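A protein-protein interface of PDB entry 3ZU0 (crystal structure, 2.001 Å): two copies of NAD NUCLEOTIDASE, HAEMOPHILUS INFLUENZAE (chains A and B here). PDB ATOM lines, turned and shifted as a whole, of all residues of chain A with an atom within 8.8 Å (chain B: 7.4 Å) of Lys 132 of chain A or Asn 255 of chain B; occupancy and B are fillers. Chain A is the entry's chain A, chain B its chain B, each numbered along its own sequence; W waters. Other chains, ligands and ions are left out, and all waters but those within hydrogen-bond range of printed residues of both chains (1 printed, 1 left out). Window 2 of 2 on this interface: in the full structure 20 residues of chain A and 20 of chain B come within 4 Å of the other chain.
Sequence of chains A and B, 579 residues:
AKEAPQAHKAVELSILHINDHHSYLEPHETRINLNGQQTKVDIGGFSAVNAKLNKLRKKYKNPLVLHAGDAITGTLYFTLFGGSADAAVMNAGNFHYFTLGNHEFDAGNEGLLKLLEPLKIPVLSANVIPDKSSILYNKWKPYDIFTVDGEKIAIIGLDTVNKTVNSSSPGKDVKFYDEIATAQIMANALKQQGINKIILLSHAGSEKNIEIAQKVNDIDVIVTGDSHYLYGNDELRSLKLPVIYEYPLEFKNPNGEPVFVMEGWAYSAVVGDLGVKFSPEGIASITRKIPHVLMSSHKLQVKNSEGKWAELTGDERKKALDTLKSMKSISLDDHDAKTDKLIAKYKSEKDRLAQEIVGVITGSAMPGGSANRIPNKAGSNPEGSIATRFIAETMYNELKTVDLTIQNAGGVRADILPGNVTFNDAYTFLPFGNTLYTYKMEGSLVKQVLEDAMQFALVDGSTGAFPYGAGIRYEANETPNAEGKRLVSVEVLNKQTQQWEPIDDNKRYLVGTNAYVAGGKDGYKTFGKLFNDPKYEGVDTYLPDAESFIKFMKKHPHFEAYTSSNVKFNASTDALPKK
The side-chain carboxylate of Asp 131 of chain A is in hydrogen-bond range of the side-chain amide nitrogen of Asn 217 of chain B, at 3.2 Å.
The backbone NH (N) of Lys 132 of chain A is in hydrogen-bond range of the side-chain amide oxygen (OD1) of Asn 255 of chain B, at 2.9 Å.
OH of Tyr 137 of chain A is in hydrogen-bond range of NZ of Lys 191 of chain B (3.5 Å).
The backbone carbonyl oxygen (O) of Lys 175 of chain A is in hydrogen-bond range of the backbone NH (N) of Ile 129 of chain A, 2.9 Å away.
The side-chain carboxylate (OD2) of Asp 131 of chain A is in salt-bridge range of the side-chain amino group (NZ) of Lys 175 of chain A.
The backbone NH of Asn 217 of chain B lies within hydrogen-bond range of the side-chain amide oxygen of Gln 184 of chain B, 2.9 Å away.
The side-chain amide oxygen (OD1) of Asn 217 of chain B lies close to the side-chain amide oxygen (OD1) of Asn 253 of chain B (3.4 Å).
OD1 of Asn 217 of chain B lies within hydrogen-bond range of N of Asn 255 of chain B, 2.8 Å away.
OD1 of Asn 253 of chain B lies within hydrogen-bond range of N of Asn 255 of chain B.
Among the printed residues, pairs that only touch across the chains: Ile 129 of chain A with Gln 184 of chain B (3.8 Å) and Asp 131 of chain A with Asn 255 of chain B (3.4 Å).
Of the printed residues of chain A, Asn 255 of chain B touches Asp 131 (3.4 Å) and Lys 132 (2.9 Å).
No residue of chain A comes within 4 Å of Pro 254 of chain B.
No residue of chain A comes within 4 Å of Gly 256 of chain B.
Of the printed residues of chain A, Lys 191 of chain B touches Tyr 137.
Printed residues of chain B within 4 Å of Ile 129 of chain A: Gln 184 (3.8 Å).
Of the printed residues of chain B, Asp 131 of chain A touches Asn 217 and Asn 255.
Of the printed residues of chain A, Asn 217 of chain B touches Asp 131 (3.2 Å).
Printed residues of chain A within 4 Å of Gln 184 of chain B: Ile 129.
Leu 136 of chain A touches none of the printed residues of chain B.
Of the 13 printed residues of chain A, 4 touch a printed residue of chain B.
Printed residues of chain A that touch a printed residue of chain B: Ile 129, Asp 131, Lys 132 and Tyr 137.
Of the 14 printed residues of chain B, 4 touch a printed residue of chain A.
Among the printed residues, no Asp or Glu carboxylate lies within 4 Å of a Lys or Arg side-chain nitrogen of the other chain.
No position is printed for both chains.
Water W1 lies within hydrogen-bond range of the side-chain hydroxyl (OG) of Ser 133 of chain A (2.9 Å), the side-chain amide oxygen (OD1) of Asn 255 of chain B (3.2 Å) and the backbone NH (N) of Lys 132 of chain A (3.3 Å).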
ATOM      1  N   ILE A 129       9.660 -22.348   1.861  1.00  0.00           N
ATOM      2  CA  ILE A 129      10.353 -23.584   2.183  1.00  0.00           C
ATOM      3  C   ILE A 129      11.484 -23.292   3.148  1.00  0.00           C
ATOM      4  O   ILE A 129      12.428 -22.573   2.804  1.00  0.00           O
ATOM      5  CB  ILE A 129      10.935 -24.230   0.903  1.00  0.00           C
ATOM      6  CG1 ILE A 129       9.839 -24.406  -0.150  1.00  0.00           C
ATOM      7  CG2 ILE A 129      11.611 -25.555   1.230  1.00  0.00           C
ATOM      8  CD1 ILE A 129      10.362 -24.909  -1.500  1.00  0.00           C
ATOM      9  N   PRO A 130      11.383 -23.822   4.374  1.00  0.00           N
ATOM     10  CA  PRO A 130      12.411 -23.565   5.389  1.00  0.00           C
ATOM     11  C   PRO A 130      13.638 -24.452   5.202  1.00  0.00           C
ATOM     12  O   PRO A 130      13.490 -25.630   4.859  1.00  0.00           O
ATOM     13  CB  PRO A 130      11.718 -23.944   6.702  1.00  0.00           C
ATOM     14  CG  PRO A 130      10.294 -24.270   6.351  1.00  0.00           C
ATOM     15  CD  PRO A 130      10.284 -24.636   4.909  1.00  0.00           C
ATOM     16  N   ASP A 131      14.827 -23.902   5.439  1.00  0.00           N
ATOM     17  CA  ASP A 131      16.035 -24.721   5.507  1.00  0.00           C
ATOM     18  C   ASP A 131      15.936 -25.698   6.684  1.00  0.00           C
ATOM     19  O   ASP A 131      15.153 -25.488   7.617  1.00  0.00           O
ATOM     20  CB  ASP A 131      17.307 -23.863   5.622  1.00  0.00           C
ATOM     21  CG  ASP A 131      17.577 -23.008   4.361  1.00  0.00           C
ATOM     22  OD1 ASP A 131      17.139 -23.361   3.249  1.00  0.00           O
ATOM     23  OD2 ASP A 131      18.243 -21.969   4.484  1.00  0.00           O
ATOM     24  N   LYS A 132      16.742 -26.756   6.629  1.00  0.00           N
ATOM     25  CA  LYS A 132      16.759 -27.813   7.635  1.00  0.00           C
ATOM     26  C   LYS A 132      17.075 -27.324   9.048  1.00  0.00           C
ATOM     27  O   LYS A 132      16.693 -27.958  10.021  1.00  0.00           O
ATOM     28  CB  LYS A 132      17.781 -28.872   7.219  1.00  0.00           C
ATOM     29  CG  LYS A 132      18.214 -29.815   8.308  1.00  0.00           C
ATOM     30  CD  LYS A 132      19.341 -30.709   7.814  1.00  0.00           C
ATOM     31  CE  LYS A 132      19.759 -31.721   8.874  1.00  0.00           C
ATOM     32  NZ  LYS A 132      18.653 -32.676   9.224  1.00  0.00           N
ATOM     33  N   SER A 133      17.766 -26.191   9.148  1.00  0.00           N
ATOM     34  CA  SER A 133      18.187 -25.658  10.438  1.00  0.00           C
ATOM     35  C   SER A 133      17.162 -24.678  11.005  1.00  0.00           C
ATOM     36  O   SER A 133      17.314 -24.194  12.118  1.00  0.00           O
ATOM     37  CB  SER A 133      19.532 -24.940  10.300  1.00  0.00           C
ATOM     38  OG  SER A 133      19.441 -23.886   9.344  1.00  0.00           O
ATOM     39  N   SER A 134      16.135 -24.373  10.221  1.00  0.00           N
ATOM     40  CA  SER A 134      15.070 -23.488  10.660  1.00  0.00           C
ATOM     41  C   SER A 134      14.261 -24.138  11.771  1.00  0.00           C
ATOM     42  O   SER A 134      13.996 -25.342  11.743  1.00  0.00           O
ATOM     43  CB  SER A 134      14.134 -23.190   9.496  1.00  0.00           C
ATOM     44  OG  SER A 134      13.245 -22.143   9.819  1.00  0.00           O
ATOM     45  N   ILE A 135      13.833 -23.336  12.737  1.00  0.00           N
ATOM     46  CA  ILE A 135      12.909 -23.841  13.751  1.00  0.00           C
ATOM     47  C   ILE A 135      11.575 -24.174  13.100  1.00  0.00           C
ATOM     48  O   ILE A 135      10.746 -24.892  13.678  1.00  0.00           O
ATOM     49  CB  ILE A 135      12.712 -22.819  14.911  1.00  0.00           C
ATOM     50  CG1 ILE A 135      12.019 -21.555  14.396  1.00  0.00           C
ATOM     51  CG2 ILE A 135      14.053 -22.501  15.559  1.00  0.00           C
ATOM     52  CD1 ILE A 135      11.950 -20.429  15.411  1.00  0.00           C
ATOM     53  N   LEU A 136      11.365 -23.662  11.884  1.00  0.00           N
ATOM     54  CA  LEU A 136      10.124 -23.946  11.149  1.00  0.00           C
ATOM     55  C   LEU A 136      10.234 -25.155  10.229  1.00  0.00           C
ATOM     56  O   LEU A 136       9.288 -25.479   9.508  1.00  0.00           O
ATOM     57  CB  LEU A 136       9.689 -22.734  10.336  1.00  0.00           C
ATOM     58  CG  LEU A 136       9.417 -21.487  11.181  1.00  0.00           C
ATOM     59  CD1 LEU A 136       8.986 -20.335  10.288  1.00  0.00           C
ATOM     60  CD2 LEU A 136       8.370 -21.788  12.238  1.00  0.00           C
ATOM     61  N   TYR A 137      11.380 -25.826  10.249  1.00  0.00           N
ATOM     62  CA  TYR A 137      11.552 -27.002   9.413  1.00  0.00           C
ATOM     63  C   TYR A 137      10.510 -28.065   9.781  1.00  0.00           C
ATOM     64  O   TYR A 137      10.207 -28.276  10.961  1.00  0.00           O
ATOM     65  CB  TYR A 137      12.977 -27.559   9.547  1.00  0.00           C
ATOM     66  CG  TYR A 137      13.271 -28.697   8.599  1.00  0.00           C
ATOM     67  CD1 TYR A 137      13.375 -28.476   7.225  1.00  0.00           C
ATOM     68  CD2 TYR A 137      13.437 -29.994   9.067  1.00  0.00           C
ATOM     69  CE1 TYR A 137      13.649 -29.517   6.351  1.00  0.00           C
ATOM     70  CE2 TYR A 137      13.712 -31.040   8.199  1.00  0.00           C
ATOM     71  CZ  TYR A 137      13.812 -30.794   6.844  1.00  0.00           C
ATOM     72  OH  TYR A 137      14.070 -31.830   5.981  1.00  0.00           O
ATOM     73  N   ASN A 138       9.945 -28.704   8.761  1.00  0.00           N
ATOM     74  CA  ASN A 138       8.933 -29.754   8.927  1.00  0.00           C
ATOM     75  C   ASN A 138       7.691 -29.351   9.724  1.00  0.00           C
ATOM     76  O   ASN A 138       7.127 -30.151  10.467  1.00  0.00           O
ATOM     77  CB  ASN A 138       9.558 -31.030   9.504  1.00  0.00           C
ATOM     78  CG  ASN A 138      10.361 -31.811   8.457  1.00  0.00           C
ATOM     79  OD1 ASN A 138      10.149 -31.656   7.241  1.00  0.00           O
ATOM     80  ND2 ASN A 138      11.283 -32.658   8.924  1.00  0.00           N
ATOM     81  N   ASP A 173      16.334 -18.021   6.895  1.00  0.00           N
ATOM     82  CA  ASP A 173      16.397 -19.441   6.607  1.00  0.00           C
ATOM     83  C   ASP A 173      15.075 -19.953   6.004  1.00  0.00           C
ATOM     84  O   ASP A 173      14.882 -21.160   5.860  1.00  0.00           O
ATOM     85  CB  ASP A 173      16.818 -20.224   7.855  1.00  0.00           C
ATOM     86  CG  ASP A 173      15.826 -20.087   9.000  1.00  0.00           C
ATOM     87  OD1 ASP A 173      14.614 -19.973   8.723  1.00  0.00           O
ATOM     88  OD2 ASP A 173      16.253 -20.082  10.186  1.00  0.00           O
ATOM     89  N   VAL A 174      14.181 -19.030   5.642  1.00  0.00           N
ATOM     90  CA  VAL A 174      12.930 -19.365   4.941  1.00  0.00           C
ATOM     91  C   VAL A 174      12.959 -18.806   3.522  1.00  0.00           C
ATOM     92  O   VAL A 174      13.008 -17.596   3.331  1.00  0.00           O
ATOM     93  CB  VAL A 174      11.685 -18.823   5.691  1.00  0.00           C
ATOM     94  CG1 VAL A 174      10.402 -19.180   4.941  1.00  0.00           C
ATOM     95  CG2 VAL A 174      11.621 -19.387   7.119  1.00  0.00           C
ATOM     96  N   LYS A 175      12.925 -19.691   2.526  1.00  0.00           N
ATOM     97  CA  LYS A 175      13.061 -19.301   1.115  1.00  0.00           C
ATOM     98  C   LYS A 175      11.709 -19.205   0.424  1.00  0.00           C
ATOM     99  O   LYS A 175      10.863 -20.077   0.610  1.00  0.00           O
ATOM    100  CB  LYS A 175      13.904 -20.347   0.374  1.00  0.00           C
ATOM    101  CG  LYS A 175      15.408 -20.076   0.349  1.00  0.00           C
ATOM    102  CD  LYS A 175      15.971 -19.907   1.729  1.00  0.00           C
ATOM    103  CE  LYS A 175      17.472 -19.623   1.670  1.00  0.00           C
ATOM    104  NZ  LYS A 175      17.967 -19.279   3.030  1.00  0.00           N
ATOM    105  N   GLN B 184      13.923 -26.605  -7.135  1.00  0.00           N
ATOM    106  CA  GLN B 184      13.574 -26.610  -5.712  1.00  0.00           C
ATOM    107  C   GLN B 184      12.147 -27.098  -5.478  1.00  0.00           C
ATOM    108  O   GLN B 184      11.907 -27.928  -4.591  1.00  0.00           O
ATOM    109  CB  GLN B 184      13.738 -25.223  -5.094  1.00  0.00           C
ATOM    110  CG  GLN B 184      13.546 -25.207  -3.543  1.00  0.00           C
ATOM    111  CD  GLN B 184      14.489 -26.144  -2.787  1.00  0.00           C
ATOM    112  OE1 GLN B 184      15.551 -25.734  -2.350  1.00  0.00           O
ATOM    113  NE2 GLN B 184      14.096 -27.393  -2.625  1.00  0.00           N
ATOM    114  N   LYS B 191       9.827 -35.013  -1.383  1.00  0.00           N
ATOM    115  CA  LYS B 191      10.177 -35.410  -0.016  1.00  0.00           C
ATOM    116  C   LYS B 191       9.090 -36.206   0.709  1.00  0.00           C
ATOM    117  O   LYS B 191       9.392 -37.144   1.446  1.00  0.00           O
ATOM    118  CB  LYS B 191      10.530 -34.190   0.844  1.00  0.00           C
ATOM    119  CG  LYS B 191      11.836 -33.491   0.497  1.00  0.00           C
ATOM    120  CD  LYS B 191      11.908 -32.117   1.193  1.00  0.00           C
ATOM    121  CE  LYS B 191      11.879 -32.244   2.716  1.00  0.00           C
ATOM    122  NZ  LYS B 191      11.921 -30.900   3.397  1.00  0.00           N
ATOM    123  N   GLN B 214      24.307 -24.948  -5.184  1.00  0.00           N
ATOM    124  CA  GLN B 214      24.640 -24.126  -4.026  1.00  0.00           C
ATOM    125  C   GLN B 214      23.412 -23.408  -3.474  1.00  0.00           C
ATOM    126  O   GLN B 214      23.452 -22.898  -2.369  1.00  0.00           O
ATOM    127  CB  GLN B 214      25.709 -23.106  -4.420  1.00  0.00           C
ATOM    128  CG  GLN B 214      27.040 -23.734  -4.840  1.00  0.00           C
ATOM    129  CD  GLN B 214      27.985 -22.727  -5.453  1.00  0.00           C
ATOM    130  OE1 GLN B 214      27.981 -22.511  -6.666  1.00  0.00           O
ATOM    131  NE2 GLN B 214      28.804 -22.111  -4.624  1.00  0.00           N
ATOM    132  N   VAL B 216      19.892 -24.674  -3.971  1.00  0.00           N
ATOM    133  CA  VAL B 216      18.720 -25.539  -3.869  1.00  0.00           C
ATOM    134  C   VAL B 216      19.030 -26.753  -2.991  1.00  0.00           C
ATOM    135  O   VAL B 216      20.122 -27.327  -3.079  1.00  0.00           O
ATOM    136  CB  VAL B 216      18.277 -26.015  -5.274  1.00  0.00           C
ATOM    137  CG1 VAL B 216      17.127 -27.012  -5.187  1.00  0.00           C
ATOM    138  CG2 VAL B 216      17.875 -24.819  -6.121  1.00  0.00           C
ATOM    139  N   ASN B 217      18.074 -27.139  -2.143  1.00  0.00           N
ATOM    140  CA  ASN B 217      18.241 -28.274  -1.229  1.00  0.00           C
ATOM    141  C   ASN B 217      17.635 -29.562  -1.758  1.00  0.00           C
ATOM    142  O   ASN B 217      16.821 -29.539  -2.675  1.00  0.00           O
ATOM    143  CB  ASN B 217      17.581 -27.971   0.107  1.00  0.00           C
ATOM    144  CG  ASN B 217      18.369 -27.003   0.934  1.00  0.00           C
ATOM    145  OD1 ASN B 217      19.564 -27.184   1.137  1.00  0.00           O
ATOM    146  ND2 ASN B 217      17.704 -25.963   1.423  1.00  0.00           N
ATOM    147  N   ASP B 218      18.032 -30.690  -1.179  1.00  0.00           N
ATOM    148  CA  ASP B 218      17.360 -31.955  -1.428  1.00  0.00           C
ATOM    149  C   ASP B 218      17.756 -32.622  -2.758  1.00  0.00           C
ATOM    150  O   ASP B 218      17.234 -33.687  -3.104  1.00  0.00           O
ATOM    151  CB  ASP B 218      15.834 -31.774  -1.354  1.00  0.00           C
ATOM    152  CG  ASP B 218      15.392 -30.983  -0.119  1.00  0.00           C
ATOM    153  OD1 ASP B 218      15.816 -31.333   1.007  1.00  0.00           O
ATOM    154  OD2 ASP B 218      14.626 -29.996  -0.284  1.00  0.00           O
ATOM    155  N   LYS B 252      28.290 -27.836  -1.333  1.00  0.00           N
ATOM    156  CA  LYS B 252      27.326 -28.029  -0.247  1.00  0.00           C
ATOM    157  C   LYS B 252      26.093 -27.195  -0.552  1.00  0.00           C
ATOM    158  O   LYS B 252      26.215 -26.039  -0.941  1.00  0.00           O
ATOM    159  CB  LYS B 252      27.904 -27.572   1.104  1.00  0.00           C
ATOM    160  CG  LYS B 252      29.213 -28.239   1.495  1.00  0.00           C
ATOM    161  CD  LYS B 252      29.046 -29.752   1.625  1.00  0.00           C
ATOM    162  CE  LYS B 252      30.236 -30.380   2.355  1.00  0.00           C
ATOM    163  NZ  LYS B 252      31.525 -30.060   1.665  1.00  0.00           N
ATOM    164  N   ASN B 253      24.910 -27.775  -0.394  1.00  0.00           N
ATOM    165  CA  ASN B 253      23.691 -27.005  -0.589  1.00  0.00           C
ATOM    166  C   ASN B 253      23.417 -26.145   0.656  1.00  0.00           C
ATOM    167  O   ASN B 253      24.193 -26.181   1.592  1.00  0.00           O
ATOM    168  CB  ASN B 253      22.509 -27.921  -0.956  1.00  0.00           C
ATOM    169  CG  ASN B 253      22.175 -28.933   0.125  1.00  0.00           C
ATOM    170  OD1 ASN B 253      22.559 -28.772   1.285  1.00  0.00           O
ATOM    171  ND2 ASN B 253      21.446 -29.996  -0.258  1.00  0.00           N
ATOM    172  N   PRO B 254      22.334 -25.350   0.657  1.00  0.00           N
ATOM    173  CA  PRO B 254      22.105 -24.534   1.862  1.00  0.00           C
ATOM    174  C   PRO B 254      21.943 -25.352   3.150  1.00  0.00           C
ATOM    175  O   PRO B 254      22.221 -24.840   4.217  1.00  0.00           O
ATOM    176  CB  PRO B 254      20.816 -23.780   1.534  1.00  0.00           C
ATOM    177  CG  PRO B 254      20.866 -23.639   0.031  1.00  0.00           C
ATOM    178  CD  PRO B 254      21.471 -24.930  -0.469  1.00  0.00           C
ATOM    179  N   ASN B 255      21.499 -26.596   3.054  1.00  0.00           N
ATOM    180  CA  ASN B 255      21.345 -27.424   4.249  1.00  0.00           C
ATOM    181  C   ASN B 255      22.643 -28.075   4.679  1.00  0.00           C
ATOM    182  O   ASN B 255      22.678 -28.806   5.655  1.00  0.00           O
ATOM    183  CB  ASN B 255      20.280 -28.492   4.042  1.00  0.00           C
ATOM    184  CG  ASN B 255      18.891 -27.910   4.038  1.00  0.00           C
ATOM    185  OD1 ASN B 255      18.706 -26.757   4.436  1.00  0.00           O
ATOM    186  ND2 ASN B 255      17.907 -28.687   3.585  1.00  0.00           N
ATOM    187  N   GLY B 256      23.702 -27.806   3.925  1.00  0.00           N
ATOM    188  CA  GLY B 256      25.014 -28.333   4.229  1.00  0.00           C
ATOM    189  C   GLY B 256      25.268 -29.686   3.605  1.00  0.00           C
ATOM    190  O   GLY B 256      26.327 -30.263   3.816  1.00  0.00           O
ATOM    191  N   GLU B 257      24.311 -30.193   2.830  1.00  0.00           N
ATOM    192  CA  GLU B 257      24.458 -31.516   2.222  1.00  0.00           C
ATOM    193  C   GLU B 257      25.298 -31.474   0.933  1.00  0.00           C
ATOM    194  O   GLU B 257      25.267 -30.486   0.196  1.00  0.00           O
ATOM    195  CB  GLU B 257      23.083 -32.134   1.942  1.00  0.00           C
ATOM    196  CG  GLU B 257      22.186 -32.319   3.195  1.00  0.00           C
ATOM    197  CD  GLU B 257      20.747 -32.633   2.812  1.00  0.00           C
ATOM    198  OE1 GLU B 257      20.186 -31.914   1.950  1.00  0.00           O
ATOM    199  OE2 GLU B 257      20.167 -33.604   3.363  1.00  0.00           O
ATOM    200  N   PRO B 258      26.034 -32.562   0.655  1.00  0.00           N
ATOM    201  CA  PRO B 258      26.879 -32.649  -0.538  1.00  0.00           C
ATOM    202  C   PRO B 258      26.036 -32.697  -1.810  1.00  0.00           C
ATOM    203  O   PRO B 258      24.996 -33.363  -1.851  1.00  0.00           O
ATOM    204  CB  PRO B 258      27.604 -33.988  -0.360  1.00  0.00           C
ATOM    205  CG  PRO B 258      27.461 -34.342   1.096  1.00  0.00           C
ATOM    206  CD  PRO B 258      26.144 -33.769   1.501  1.00  0.00           C
ATOM    207  N   ILE B 283      22.313 -39.136   1.992  1.00  0.00           N
ATOM    208  CA  ILE B 283      23.498 -38.303   1.790  1.00  0.00           C
ATOM    209  C   ILE B 283      24.434 -39.040   0.836  1.00  0.00           C
ATOM    210  O   ILE B 283      24.792 -40.195   1.076  1.00  0.00           O
ATOM    211  CB  ILE B 283      24.216 -38.007   3.128  1.00  0.00           C
ATOM    212  CG1 ILE B 283      23.364 -37.098   4.029  1.00  0.00           C
ATOM    213  CG2 ILE B 283      25.595 -37.392   2.898  1.00  0.00           C
ATOM    214  CD1 ILE B 283      23.222 -35.677   3.530  1.00  0.00           C
HETATM  215  O   HOH W   1      19.843 -25.715   7.192  1.00  0.00           O
